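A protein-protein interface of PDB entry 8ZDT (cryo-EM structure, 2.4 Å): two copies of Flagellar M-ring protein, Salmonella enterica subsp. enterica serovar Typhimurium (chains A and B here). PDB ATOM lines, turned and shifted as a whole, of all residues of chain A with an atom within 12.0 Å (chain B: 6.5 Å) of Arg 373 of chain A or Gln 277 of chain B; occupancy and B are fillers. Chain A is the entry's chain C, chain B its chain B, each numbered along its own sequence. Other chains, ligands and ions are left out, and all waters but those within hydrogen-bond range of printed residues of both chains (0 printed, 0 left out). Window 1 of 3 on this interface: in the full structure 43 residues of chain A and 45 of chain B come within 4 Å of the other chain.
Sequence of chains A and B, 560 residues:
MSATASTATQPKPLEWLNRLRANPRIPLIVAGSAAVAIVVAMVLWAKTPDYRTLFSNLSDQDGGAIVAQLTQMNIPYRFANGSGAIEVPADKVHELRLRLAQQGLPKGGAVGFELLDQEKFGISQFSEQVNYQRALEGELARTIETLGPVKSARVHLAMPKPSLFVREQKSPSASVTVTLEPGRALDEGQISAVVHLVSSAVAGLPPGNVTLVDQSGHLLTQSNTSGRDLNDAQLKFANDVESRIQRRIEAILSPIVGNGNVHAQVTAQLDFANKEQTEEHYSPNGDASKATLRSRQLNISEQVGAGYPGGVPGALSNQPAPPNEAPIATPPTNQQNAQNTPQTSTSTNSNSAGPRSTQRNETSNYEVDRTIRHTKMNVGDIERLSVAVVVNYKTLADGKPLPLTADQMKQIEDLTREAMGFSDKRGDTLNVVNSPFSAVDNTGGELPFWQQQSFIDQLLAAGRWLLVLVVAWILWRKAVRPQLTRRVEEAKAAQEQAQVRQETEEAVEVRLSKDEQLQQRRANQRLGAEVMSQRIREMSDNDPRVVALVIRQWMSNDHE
N of Thr 278 of chain B sits at hydrogen-bond distance from O of Ile 372 of chain A (3.1 Å).
NE2 of Gln 277 of chain B lies close to NH1 of Arg 373 of chain A (3.0 Å).
The backbone NH (N) of Glu 276 of chain B sits at hydrogen-bond distance from the backbone carbonyl oxygen (O) of His 374 of chain A, 3.1 Å away.
The side-chain carboxylate of Glu 279 of chain B sits close to the side-chain amide oxygen of Gln 277 of chain B (3.1 Å).
The backbone NH (N) of Met 377 of chain B lies within hydrogen-bond range of the backbone carbonyl oxygen (O) of Lys 275 of chain B (3.1 Å).
N of Glu 279 of chain A sits at hydrogen-bond distance from O of Arg 373 of chain A (2.9 Å).
N of Gln 277 of chain B lies within hydrogen-bond range of O of Thr 375 of chain B (2.9 Å).
The backbone NH of Gln 277 of chain A lies within hydrogen-bond range of the backbone carbonyl oxygen of Thr 375 of chain A (2.9 Å).
N of His 281 of chain A is in hydrogen-bond range of O of Thr 371 of chain A (2.9 Å).
CA of Thr 371 of chain A touches O of Thr 278 of chain B, 3.5 Å away.
O of Ile 372 of chain A touches CA of Gln 277 of chain B (3.5 Å).
Arg 373 of chain A touches Lys 275 of chain B (NH2 to CD, 3.5 Å).
Arg 373 of chain A touches Glu 276 of chain B.
O of His 374 of chain A touches CA of Lys 275 of chain B, 3.4 Å away.
Thr 375 of chain A touches Lys 275 of chain B.
Gln 277 of chain B touches just these residues of chain A: Ile 372 and Arg 373.
Glu 276 of chain B touches just these residues of chain A: Arg 373 and His 374.
No residue of chain A comes within 4 Å of Glu 279 of chain B.
No residue of chain A comes within 4 Å of His 374 of chain B.
Of the printed residues of chain B, Ile 372 of chain A touches Gln 277 and Thr 278.
Of the printed residues of chain B, Thr 371 of chain A touches Thr 278 (3.5 Å).
Of the printed residues of chain B, His 374 of chain A touches Lys 275 (3.4 Å) and Glu 276 (3.1 Å).
Of the printed residues of chain B, Thr 375 of chain A touches Lys 275.
Ser 283 of chain A touches none of the printed residues of chain B.
Glu 280 of chain A touches none of the printed residues of chain B.
The nearest printed residue of chain B that does not touch Thr 371 of chain A is Glu 279 of chain B (4.2 Å).
Of the 10 printed residues of chain B, 4 touch a printed residue of chain A.
Printed residues of chain B that touch a printed residue of chain A: Lys 275, Glu 276, Gln 277 and Thr 278.
Among the printed residues, 9 pairs touch across the chains.
Arg 373 of chain A touches Lys 275 of chain B, but with the chains exchanged Lys 275 of chain A does not touch Arg 373 of chain B (21.5 Å).
Arg 373 of chain A touches Glu 276 of chain B, but with the chains exchanged Glu 276 of chain A does not touch Arg 373 of chain B (19.6 Å).
Arg 373 of chain A touches Gln 277 of chain B, but with the chains exchanged Gln 277 of chain A does not touch Arg 373 of chain B (15.6 Å).
Thr 375 of chain A touches Lys 275 of chain B, but with the chains exchanged Lys 275 of chain A does not touch Thr 375 of chain B (16.5 Å).
Positions printed for both chains: 275, 276, 277, 278, 279, 373, 374, 375, 376 and 377.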
ATOM      1  N   LYS A 275      19.886 -12.328   1.992  1.00  0.00           N
ATOM      2  CA  LYS A 275      20.067 -12.817   3.349  1.00  0.00           C
ATOM      3  C   LYS A 275      21.342 -13.644   3.448  1.00  0.00           C
ATOM      4  O   LYS A 275      21.691 -14.389   2.530  1.00  0.00           O
ATOM      5  CB  LYS A 275      18.871 -13.664   3.803  1.00  0.00           C
ATOM      6  CG  LYS A 275      17.569 -12.900   3.908  1.00  0.00           C
ATOM      7  CD  LYS A 275      16.382 -13.803   3.641  1.00  0.00           C
ATOM      8  CE  LYS A 275      15.079 -13.029   3.720  1.00  0.00           C
ATOM      9  NZ  LYS A 275      14.107 -13.663   4.649  1.00  0.00           N
ATOM     10  N   GLU A 276      22.034 -13.496   4.576  1.00  0.00           N
ATOM     11  CA  GLU A 276      23.198 -14.306   4.907  1.00  0.00           C
ATOM     12  C   GLU A 276      23.074 -14.775   6.347  1.00  0.00           C
ATOM     13  O   GLU A 276      22.427 -14.123   7.169  1.00  0.00           O
ATOM     14  CB  GLU A 276      24.515 -13.538   4.729  1.00  0.00           C
ATOM     15  CG  GLU A 276      24.527 -12.550   3.581  1.00  0.00           C
ATOM     16  CD  GLU A 276      25.901 -11.962   3.342  1.00  0.00           C
ATOM     17  OE1 GLU A 276      26.901 -12.686   3.532  1.00  0.00           O
ATOM     18  OE2 GLU A 276      25.984 -10.774   2.965  1.00  0.00           O
ATOM     19  N   GLN A 277      23.699 -15.911   6.652  1.00  0.00           N
ATOM     20  CA  GLN A 277      23.604 -16.471   7.992  1.00  0.00           C
ATOM     21  C   GLN A 277      24.900 -17.180   8.359  1.00  0.00           C
ATOM     22  O   GLN A 277      25.540 -17.807   7.509  1.00  0.00           O
ATOM     23  CB  GLN A 277      22.424 -17.441   8.103  1.00  0.00           C
ATOM     24  CG  GLN A 277      21.975 -17.713   9.524  1.00  0.00           C
ATOM     25  CD  GLN A 277      20.834 -18.705   9.592  1.00  0.00           C
ATOM     26  OE1 GLN A 277      20.973 -19.793  10.149  1.00  0.00           O
ATOM     27  NE2 GLN A 277      19.695 -18.334   9.021  1.00  0.00           N
ATOM     28  N   THR A 278      25.277 -17.067   9.632  1.00  0.00           N
ATOM     29  CA  THR A 278      26.423 -17.766  10.199  1.00  0.00           C
ATOM     30  C   THR A 278      26.004 -18.397  11.518  1.00  0.00           C
ATOM     31  O   THR A 278      25.445 -17.715  12.383  1.00  0.00           O
ATOM     32  CB  THR A 278      27.606 -16.818  10.419  1.00  0.00           C
ATOM     33  OG1 THR A 278      27.999 -16.240   9.169  1.00  0.00           O
ATOM     34  CG2 THR A 278      28.787 -17.567  11.012  1.00  0.00           C
ATOM     35  N   GLU A 279      26.276 -19.690  11.672  1.00  0.00           N
ATOM     36  CA  GLU A 279      25.906 -20.444  12.861  1.00  0.00           C
ATOM     37  C   GLU A 279      27.140 -21.110  13.453  1.00  0.00           C
ATOM     38  O   GLU A 279      27.985 -21.632  12.721  1.00  0.00           O
ATOM     39  CB  GLU A 279      24.850 -21.503  12.536  1.00  0.00           C
ATOM     40  CG  GLU A 279      23.701 -20.993  11.687  1.00  0.00           C
ATOM     41  CD  GLU A 279      23.322 -21.956  10.578  1.00  0.00           C
ATOM     42  OE1 GLU A 279      23.429 -21.574   9.392  1.00  0.00           O
ATOM     43  OE2 GLU A 279      22.918 -23.097  10.891  1.00  0.00           O
ATOM     44  N   GLU A 280      27.239 -21.088  14.780  1.00  0.00           N
ATOM     45  CA  GLU A 280      28.357 -21.698  15.490  1.00  0.00           C
ATOM     46  C   GLU A 280      27.820 -22.482  16.677  1.00  0.00           C
ATOM     47  O   GLU A 280      27.015 -21.960  17.452  1.00  0.00           O
ATOM     48  CB  GLU A 280      29.356 -20.633  15.954  1.00  0.00           C
ATOM     49  CG  GLU A 280      30.493 -21.167  16.799  1.00  0.00           C
ATOM     50  CD  GLU A 280      31.543 -20.113  17.078  1.00  0.00           C
ATOM     51  OE1 GLU A 280      32.743 -20.454  17.090  1.00  0.00           O
ATOM     52  OE2 GLU A 280      31.169 -18.939  17.284  1.00  0.00           O
ATOM     53  N   HIS A 281      28.263 -23.731  16.818  1.00  0.00           N
ATOM     54  CA  HIS A 281      27.760 -24.617  17.857  1.00  0.00           C
ATOM     55  C   HIS A 281      28.906 -25.350  18.541  1.00  0.00           C
ATOM     56  O   HIS A 281      29.951 -25.611  17.938  1.00  0.00           O
ATOM     57  CB  HIS A 281      26.765 -25.639  17.291  1.00  0.00           C
ATOM     58  CG  HIS A 281      25.436 -25.054  16.929  1.00  0.00           C
ATOM     59  ND1 HIS A 281      24.990 -24.967  15.628  1.00  0.00           N
ATOM     60  CD2 HIS A 281      24.455 -24.524  17.699  1.00  0.00           C
ATOM     61  CE1 HIS A 281      23.792 -24.411  15.611  1.00  0.00           C
ATOM     62  NE2 HIS A 281      23.445 -24.132  16.856  1.00  0.00           N
ATOM     63  N   TYR A 282      28.686 -25.687  19.813  1.00  0.00           N
ATOM     64  CA  TYR A 282      29.625 -26.449  20.624  1.00  0.00           C
ATOM     65  C   TYR A 282      28.906 -27.639  21.243  1.00  0.00           C
ATOM     66  O   TYR A 282      27.697 -27.599  21.477  1.00  0.00           O
ATOM     67  CB  TYR A 282      30.241 -25.598  21.744  1.00  0.00           C
ATOM     68  CG  TYR A 282      31.164 -24.500  21.273  1.00  0.00           C
ATOM     69  CD1 TYR A 282      30.666 -23.253  20.924  1.00  0.00           C
ATOM     70  CD2 TYR A 282      32.533 -24.704  21.193  1.00  0.00           C
ATOM     71  CE1 TYR A 282      31.506 -22.243  20.500  1.00  0.00           C
ATOM     72  CE2 TYR A 282      33.381 -23.700  20.770  1.00  0.00           C
ATOM     73  CZ  TYR A 282      32.861 -22.472  20.424  1.00  0.00           C
ATOM     74  OH  TYR A 282      33.698 -21.467  20.002  1.00  0.00           O
ATOM     75  N   SER A 283      29.664 -28.703  21.508  1.00  0.00           N
ATOM     76  CA  SER A 283      29.024 -29.846  22.153  1.00  0.00           C
ATOM     77  C   SER A 283      29.159 -29.749  23.671  1.00  0.00           C
ATOM     78  O   SER A 283      30.190 -29.294  24.175  1.00  0.00           O
ATOM     79  CB  SER A 283      29.638 -31.157  21.672  1.00  0.00           C
ATOM     80  OG  SER A 283      29.549 -31.279  20.264  1.00  0.00           O
ATOM     81  N   ASP A 369      34.534 -29.498  21.024  1.00  0.00           N
ATOM     82  CA  ASP A 369      34.168 -29.691  19.626  1.00  0.00           C
ATOM     83  C   ASP A 369      33.332 -28.511  19.147  1.00  0.00           C
ATOM     84  O   ASP A 369      32.353 -28.132  19.797  1.00  0.00           O
ATOM     85  CB  ASP A 369      33.388 -30.993  19.440  1.00  0.00           C
ATOM     86  CG  ASP A 369      33.995 -32.154  20.201  1.00  0.00           C
ATOM     87  OD1 ASP A 369      35.237 -32.216  20.312  1.00  0.00           O
ATOM     88  OD2 ASP A 369      33.230 -33.013  20.684  1.00  0.00           O
ATOM     89  N   ARG A 370      33.715 -27.940  18.007  1.00  0.00           N
ATOM     90  CA  ARG A 370      33.091 -26.734  17.480  1.00  0.00           C
ATOM     91  C   ARG A 370      32.739 -26.920  16.010  1.00  0.00           C
ATOM     92  O   ARG A 370      33.536 -27.459  15.237  1.00  0.00           O
ATOM     93  CB  ARG A 370      34.022 -25.528  17.667  1.00  0.00           C
ATOM     94  CG  ARG A 370      34.000 -24.504  16.552  1.00  0.00           C
ATOM     95  CD  ARG A 370      34.566 -23.188  17.040  1.00  0.00           C
ATOM     96  NE  ARG A 370      36.015 -23.248  17.194  1.00  0.00           N
ATOM     97  CZ  ARG A 370      36.886 -22.937  16.243  1.00  0.00           C
ATOM     98  NH1 ARG A 370      36.491 -22.521  15.052  1.00  0.00           N
ATOM     99  NH2 ARG A 370      38.188 -23.045  16.496  1.00  0.00           N
ATOM    100  N   THR A 371      31.541 -26.471  15.634  1.00  0.00           N
ATOM    101  CA  THR A 371      31.056 -26.549  14.260  1.00  0.00           C
ATOM    102  C   THR A 371      30.603 -25.170  13.799  1.00  0.00           C
ATOM    103  O   THR A 371      29.876 -24.480  14.520  1.00  0.00           O
ATOM    104  CB  THR A 371      29.900 -27.545  14.141  1.00  0.00           C
ATOM    105  OG1 THR A 371      30.312 -28.821  14.643  1.00  0.00           O
ATOM    106  CG2 THR A 371      29.477 -27.699  12.690  1.00  0.00           C
ATOM    107  N   ILE A 372      31.030 -24.771  12.600  1.00  0.00           N
ATOM    108  CA  ILE A 372      30.681 -23.480  12.017  1.00  0.00           C
ATOM    109  C   ILE A 372      30.069 -23.709  10.641  1.00  0.00           C
ATOM    110  O   ILE A 372      30.611 -24.473   9.835  1.00  0.00           O
ATOM    111  CB  ILE A 372      31.899 -22.543  11.907  1.00  0.00           C
ATOM    112  CG1 ILE A 372      32.659 -22.482  13.229  1.00  0.00           C
ATOM    113  CG2 ILE A 372      31.469 -21.149  11.475  1.00  0.00           C
ATOM    114  CD1 ILE A 372      34.002 -21.813  13.113  1.00  0.00           C
ATOM    115  N   ARG A 373      28.948 -23.041  10.372  1.00  0.00           N
ATOM    116  CA  ARG A 373      28.282 -23.100   9.079  1.00  0.00           C
ATOM    117  C   ARG A 373      27.999 -21.689   8.584  1.00  0.00           C
ATOM    118  O   ARG A 373      27.587 -20.823   9.359  1.00  0.00           O
ATOM    119  CB  ARG A 373      26.975 -23.893   9.159  1.00  0.00           C
ATOM    120  CG  ARG A 373      26.434 -24.329   7.811  1.00  0.00           C
ATOM    121  CD  ARG A 373      25.176 -25.162   7.973  1.00  0.00           C
ATOM    122  NE  ARG A 373      24.571 -25.495   6.690  1.00  0.00           N
ATOM    123  CZ  ARG A 373      24.338 -26.731   6.269  1.00  0.00           C
ATOM    124  NH1 ARG A 373      24.641 -27.782   7.011  1.00  0.00           N
ATOM    125  NH2 ARG A 373      23.779 -26.915   5.076  1.00  0.00           N
ATOM    126  N   HIS A 374      28.226 -21.461   7.293  1.00  0.00           N
ATOM    127  CA  HIS A 374      27.964 -20.175   6.659  1.00  0.00           C
ATOM    128  C   HIS A 374      27.118 -20.401   5.416  1.00  0.00           C
ATOM    129  O   HIS A 374      27.453 -21.247   4.583  1.00  0.00           O
ATOM    130  CB  HIS A 374      29.268 -19.462   6.293  1.00  0.00           C
ATOM    131  CG  HIS A 374      29.066 -18.114   5.674  1.00  0.00           C
ATOM    132  ND1 HIS A 374      29.638 -17.751   4.475  1.00  0.00           N
ATOM    133  CD2 HIS A 374      28.347 -17.043   6.086  1.00  0.00           C
ATOM    134  CE1 HIS A 374      29.284 -16.514   4.176  1.00  0.00           C
ATOM    135  NE2 HIS A 374      28.501 -16.062   5.139  1.00  0.00           N
ATOM    136  N   THR A 375      26.027 -19.646   5.288  1.00  0.00           N
ATOM    137  CA  THR A 375      25.123 -19.815   4.159  1.00  0.00           C
ATOM    138  C   THR A 375      24.706 -18.463   3.601  1.00  0.00           C
ATOM    139  O   THR A 375      24.549 -17.490   4.345  1.00  0.00           O
ATOM    140  CB  THR A 375      23.877 -20.623   4.551  1.00  0.00           C
ATOM    141  OG1 THR A 375      22.871 -20.479   3.541  1.00  0.00           O
ATOM    142  CG2 THR A 375      23.327 -20.151   5.880  1.00  0.00           C
ATOM    143  N   LYS A 376      24.540 -18.414   2.281  1.00  0.00           N
ATOM    144  CA  LYS A 376      24.033 -17.243   1.577  1.00  0.00           C
ATOM    145  C   LYS A 376      22.843 -17.679   0.734  1.00  0.00           C
ATOM    146  O   LYS A 376      22.987 -18.517  -0.162  1.00  0.00           O
ATOM    147  CB  LYS A 376      25.120 -16.613   0.703  1.00  0.00           C
ATOM    148  CG  LYS A 376      24.595 -15.675  -0.366  1.00  0.00           C
ATOM    149  CD  LYS A 376      25.605 -14.586  -0.688  1.00  0.00           C
ATOM    150  CE  LYS A 376      25.724 -14.367  -2.187  1.00  0.00           C
ATOM    151  NZ  LYS A 376      24.512 -14.823  -2.922  1.00  0.00           N
ATOM    152  N   MET A 377      21.677 -17.111   1.020  1.00  0.00           N
ATOM    153  CA  MET A 377      20.438 -17.559   0.404  1.00  0.00           C
ATOM    154  C   MET A 377      20.339 -17.089  -1.045  1.00  0.00           C
ATOM    155  O   MET A 377      21.006 -16.143  -1.471  1.00  0.00           O
ATOM    156  CB  MET A 377      19.237 -17.064   1.209  1.00  0.00           C
ATOM    157  CG  MET A 377      18.553 -18.147   2.028  1.00  0.00           C
ATOM    158  SD  MET A 377      19.512 -18.679   3.461  1.00  0.00           S
ATOM    159  CE  MET A 377      19.974 -17.105   4.175  1.00  0.00           C
ATOM    160  N   LYS B 275      26.761 -22.915   0.582  1.00  0.00           N
ATOM    161  CA  LYS B 275      26.977 -23.343   1.955  1.00  0.00           C
ATOM    162  C   LYS B 275      28.377 -23.918   2.116  1.00  0.00           C
ATOM    163  O   LYS B 275      28.895 -24.598   1.226  1.00  0.00           O
ATOM    164  CB  LYS B 275      25.942 -24.390   2.385  1.00  0.00           C
ATOM    165  CG  LYS B 275      24.519 -23.880   2.429  1.00  0.00           C
ATOM    166  CD  LYS B 275      23.529 -24.990   2.140  1.00  0.00           C
ATOM    167  CE  LYS B 275      22.104 -24.469   2.158  1.00  0.00           C
ATOM    168  NZ  LYS B 275      21.231 -25.260   3.066  1.00  0.00           N
ATOM    169  N   GLU B 276      28.989 -23.628   3.263  1.00  0.00           N
ATOM    170  CA  GLU B 276      30.269 -24.204   3.651  1.00  0.00           C
ATOM    171  C   GLU B 276      30.178 -24.667   5.096  1.00  0.00           C
ATOM    172  O   GLU B 276      29.391 -24.133   5.881  1.00  0.00           O
ATOM    173  CB  GLU B 276      31.426 -23.207   3.503  1.00  0.00           C
ATOM    174  CG  GLU B 276      31.300 -22.252   2.335  1.00  0.00           C
ATOM    175  CD  GLU B 276      32.549 -21.422   2.131  1.00  0.00           C
ATOM    176  OE1 GLU B 276      33.657 -21.946   2.371  1.00  0.00           O
ATOM    177  OE2 GLU B 276      32.426 -20.245   1.732  1.00  0.00           O
ATOM    178  N   GLN B 277      30.990 -25.663   5.446  1.00  0.00           N
ATOM    179  CA  GLN B 277      30.951 -26.211   6.793  1.00  0.00           C
ATOM    180  C   GLN B 277      32.340 -26.661   7.220  1.00  0.00           C
ATOM    181  O   GLN B 277      33.116 -27.172   6.407  1.00  0.00           O
ATOM    182  CB  GLN B 277      29.966 -27.381   6.885  1.00  0.00           C
ATOM    183  CG  GLN B 277      29.522 -27.712   8.294  1.00  0.00           C
ATOM    184  CD  GLN B 277      28.582 -28.896   8.344  1.00  0.00           C
ATOM    185  OE1 GLN B 277      28.898 -29.931   8.928  1.00  0.00           O
ATOM    186  NE2 GLN B 277      27.416 -28.750   7.727  1.00  0.00           N
ATOM    187  N   THR B 278      32.641 -26.463   8.502  1.00  0.00           N
ATOM    188  CA  THR B 278      33.873 -26.930   9.123  1.00  0.00           C
ATOM    189  C   THR B 278      33.529 -27.608  10.440  1.00  0.00           C
ATOM    190  O   THR B 278      32.822 -27.030  11.270  1.00  0.00           O
ATOM    191  CB  THR B 278      34.853 -25.775   9.364  1.00  0.00           C
ATOM    192  OG1 THR B 278      35.179 -25.154   8.116  1.00  0.00           O
ATOM    193  CG2 THR B 278      36.128 -26.284  10.014  1.00  0.00           C
ATOM    194  N   GLU B 279      34.028 -28.826  10.631  1.00  0.00           N
ATOM    195  CA  GLU B 279      33.760 -29.618  11.822  1.00  0.00           C
ATOM    196  C   GLU B 279      35.073 -30.035  12.470  1.00  0.00           C
ATOM    197  O   GLU B 279      36.027 -30.403  11.779  1.00  0.00           O
ATOM    198  CB  GLU B 279      32.931 -30.860  11.483  1.00  0.00           C
ATOM    199  CG  GLU B 279      31.739 -30.583  10.584  1.00  0.00           C
ATOM    200  CD  GLU B 279      31.587 -31.616   9.483  1.00  0.00           C
ATOM    201  OE1 GLU B 279      31.667 -31.239   8.295  1.00  0.00           O
ATOM    202  OE2 GLU B 279      31.389 -32.806   9.807  1.00  0.00           O
ATOM    203  N   ARG B 373      37.321 -31.643   9.495  1.00  0.00           N
ATOM    204  CA  ARG B 373      36.727 -31.843   8.181  1.00  0.00           C
ATOM    205  C   ARG B 373      36.208 -30.515   7.647  1.00  0.00           C
ATOM    206  O   ARG B 373      35.613 -29.729   8.389  1.00  0.00           O
ATOM    207  CB  ARG B 373      35.587 -32.864   8.233  1.00  0.00           C
ATOM    208  CG  ARG B 373      35.186 -33.410   6.877  1.00  0.00           C
ATOM    209  CD  ARG B 373      34.099 -34.460   7.012  1.00  0.00           C
ATOM    210  NE  ARG B 373      33.615 -34.918   5.717  1.00  0.00           N
ATOM    211  CZ  ARG B 373      33.629 -36.181   5.314  1.00  0.00           C
ATOM    212  NH1 ARG B 373      34.093 -37.148   6.088  1.00  0.00           N
ATOM    213  NH2 ARG B 373      33.159 -36.483   4.107  1.00  0.00           N
ATOM    214  N   HIS B 374      36.437 -30.269   6.360  1.00  0.00           N
ATOM    215  CA  HIS B 374      35.966 -29.063   5.690  1.00  0.00           C
ATOM    216  C   HIS B 374      35.223 -29.458   4.424  1.00  0.00           C
ATOM    217  O   HIS B 374      35.740 -30.240   3.621  1.00  0.00           O
ATOM    218  CB  HIS B 374      37.129 -28.125   5.354  1.00  0.00           C
ATOM    219  CG  HIS B 374      36.704 -26.847   4.700  1.00  0.00           C
ATOM    220  ND1 HIS B 374      37.246 -26.402   3.514  1.00  0.00           N
ATOM    221  CD2 HIS B 374      35.786 -25.922   5.065  1.00  0.00           C
ATOM    222  CE1 HIS B 374      36.681 -25.256   3.177  1.00  0.00           C
ATOM    223  NE2 HIS B 374      35.791 -24.943   4.103  1.00  0.00           N
ATOM    224  N   THR B 375      34.018 -28.921   4.242  1.00  0.00           N
ATOM    225  CA  THR B 375      33.204 -29.270   3.087  1.00  0.00           C
ATOM    226  C   THR B 375      32.566 -28.028   2.486  1.00  0.00           C
ATOM    227  O   THR B 375      32.204 -27.090   3.204  1.00  0.00           O
ATOM    228  CB  THR B 375      32.115 -30.290   3.453  1.00  0.00           C
ATOM    229  OG1 THR B 375      31.138 -30.350   2.406  1.00  0.00           O
ATOM    230  CG2 THR B 375      31.437 -29.908   4.752  1.00  0.00           C
ATOM    231  N   LYS B 376      32.443 -28.029   1.160  1.00  0.00           N
ATOM    232  CA  LYS B 376      31.756 -26.983   0.415  1.00  0.00           C
ATOM    233  C   LYS B 376      30.700 -27.643  -0.459  1.00  0.00           C
ATOM    234  O   LYS B 376      31.031 -28.453  -1.332  1.00  0.00           O
ATOM    235  CB  LYS B 376      32.741 -26.175  -0.434  1.00  0.00           C
ATOM    236  CG  LYS B 376      32.093 -25.365  -1.541  1.00  0.00           C
ATOM    237  CD  LYS B 376      32.894 -24.113  -1.850  1.00  0.00           C
ATOM    238  CE  LYS B 376      33.029 -23.897  -3.349  1.00  0.00           C
ATOM    239  NZ  LYS B 376      31.951 -24.582  -4.115  1.00  0.00           N
ATOM    240  N   MET B 377      29.439 -27.298  -0.226  1.00  0.00           N
ATOM    241  CA  MET B 377      28.328 -27.976  -0.875  1.00  0.00           C
ATOM    242  C   MET B 377      28.199 -27.554  -2.336  1.00  0.00           C
ATOM    243  O   MET B 377      28.696 -26.507  -2.759  1.00  0.00           O
ATOM    244  CB  MET B 377      27.027 -27.701  -0.122  1.00  0.00           C
ATOM    245  CG  MET B 377      26.526 -28.880   0.695  1.00  0.00           C
ATOM    246  SD  MET B 377      27.510 -29.204   2.172  1.00  0.00           S
ATOM    247  CE  MET B 377      27.645 -27.562   2.868  1.00  0.00           C
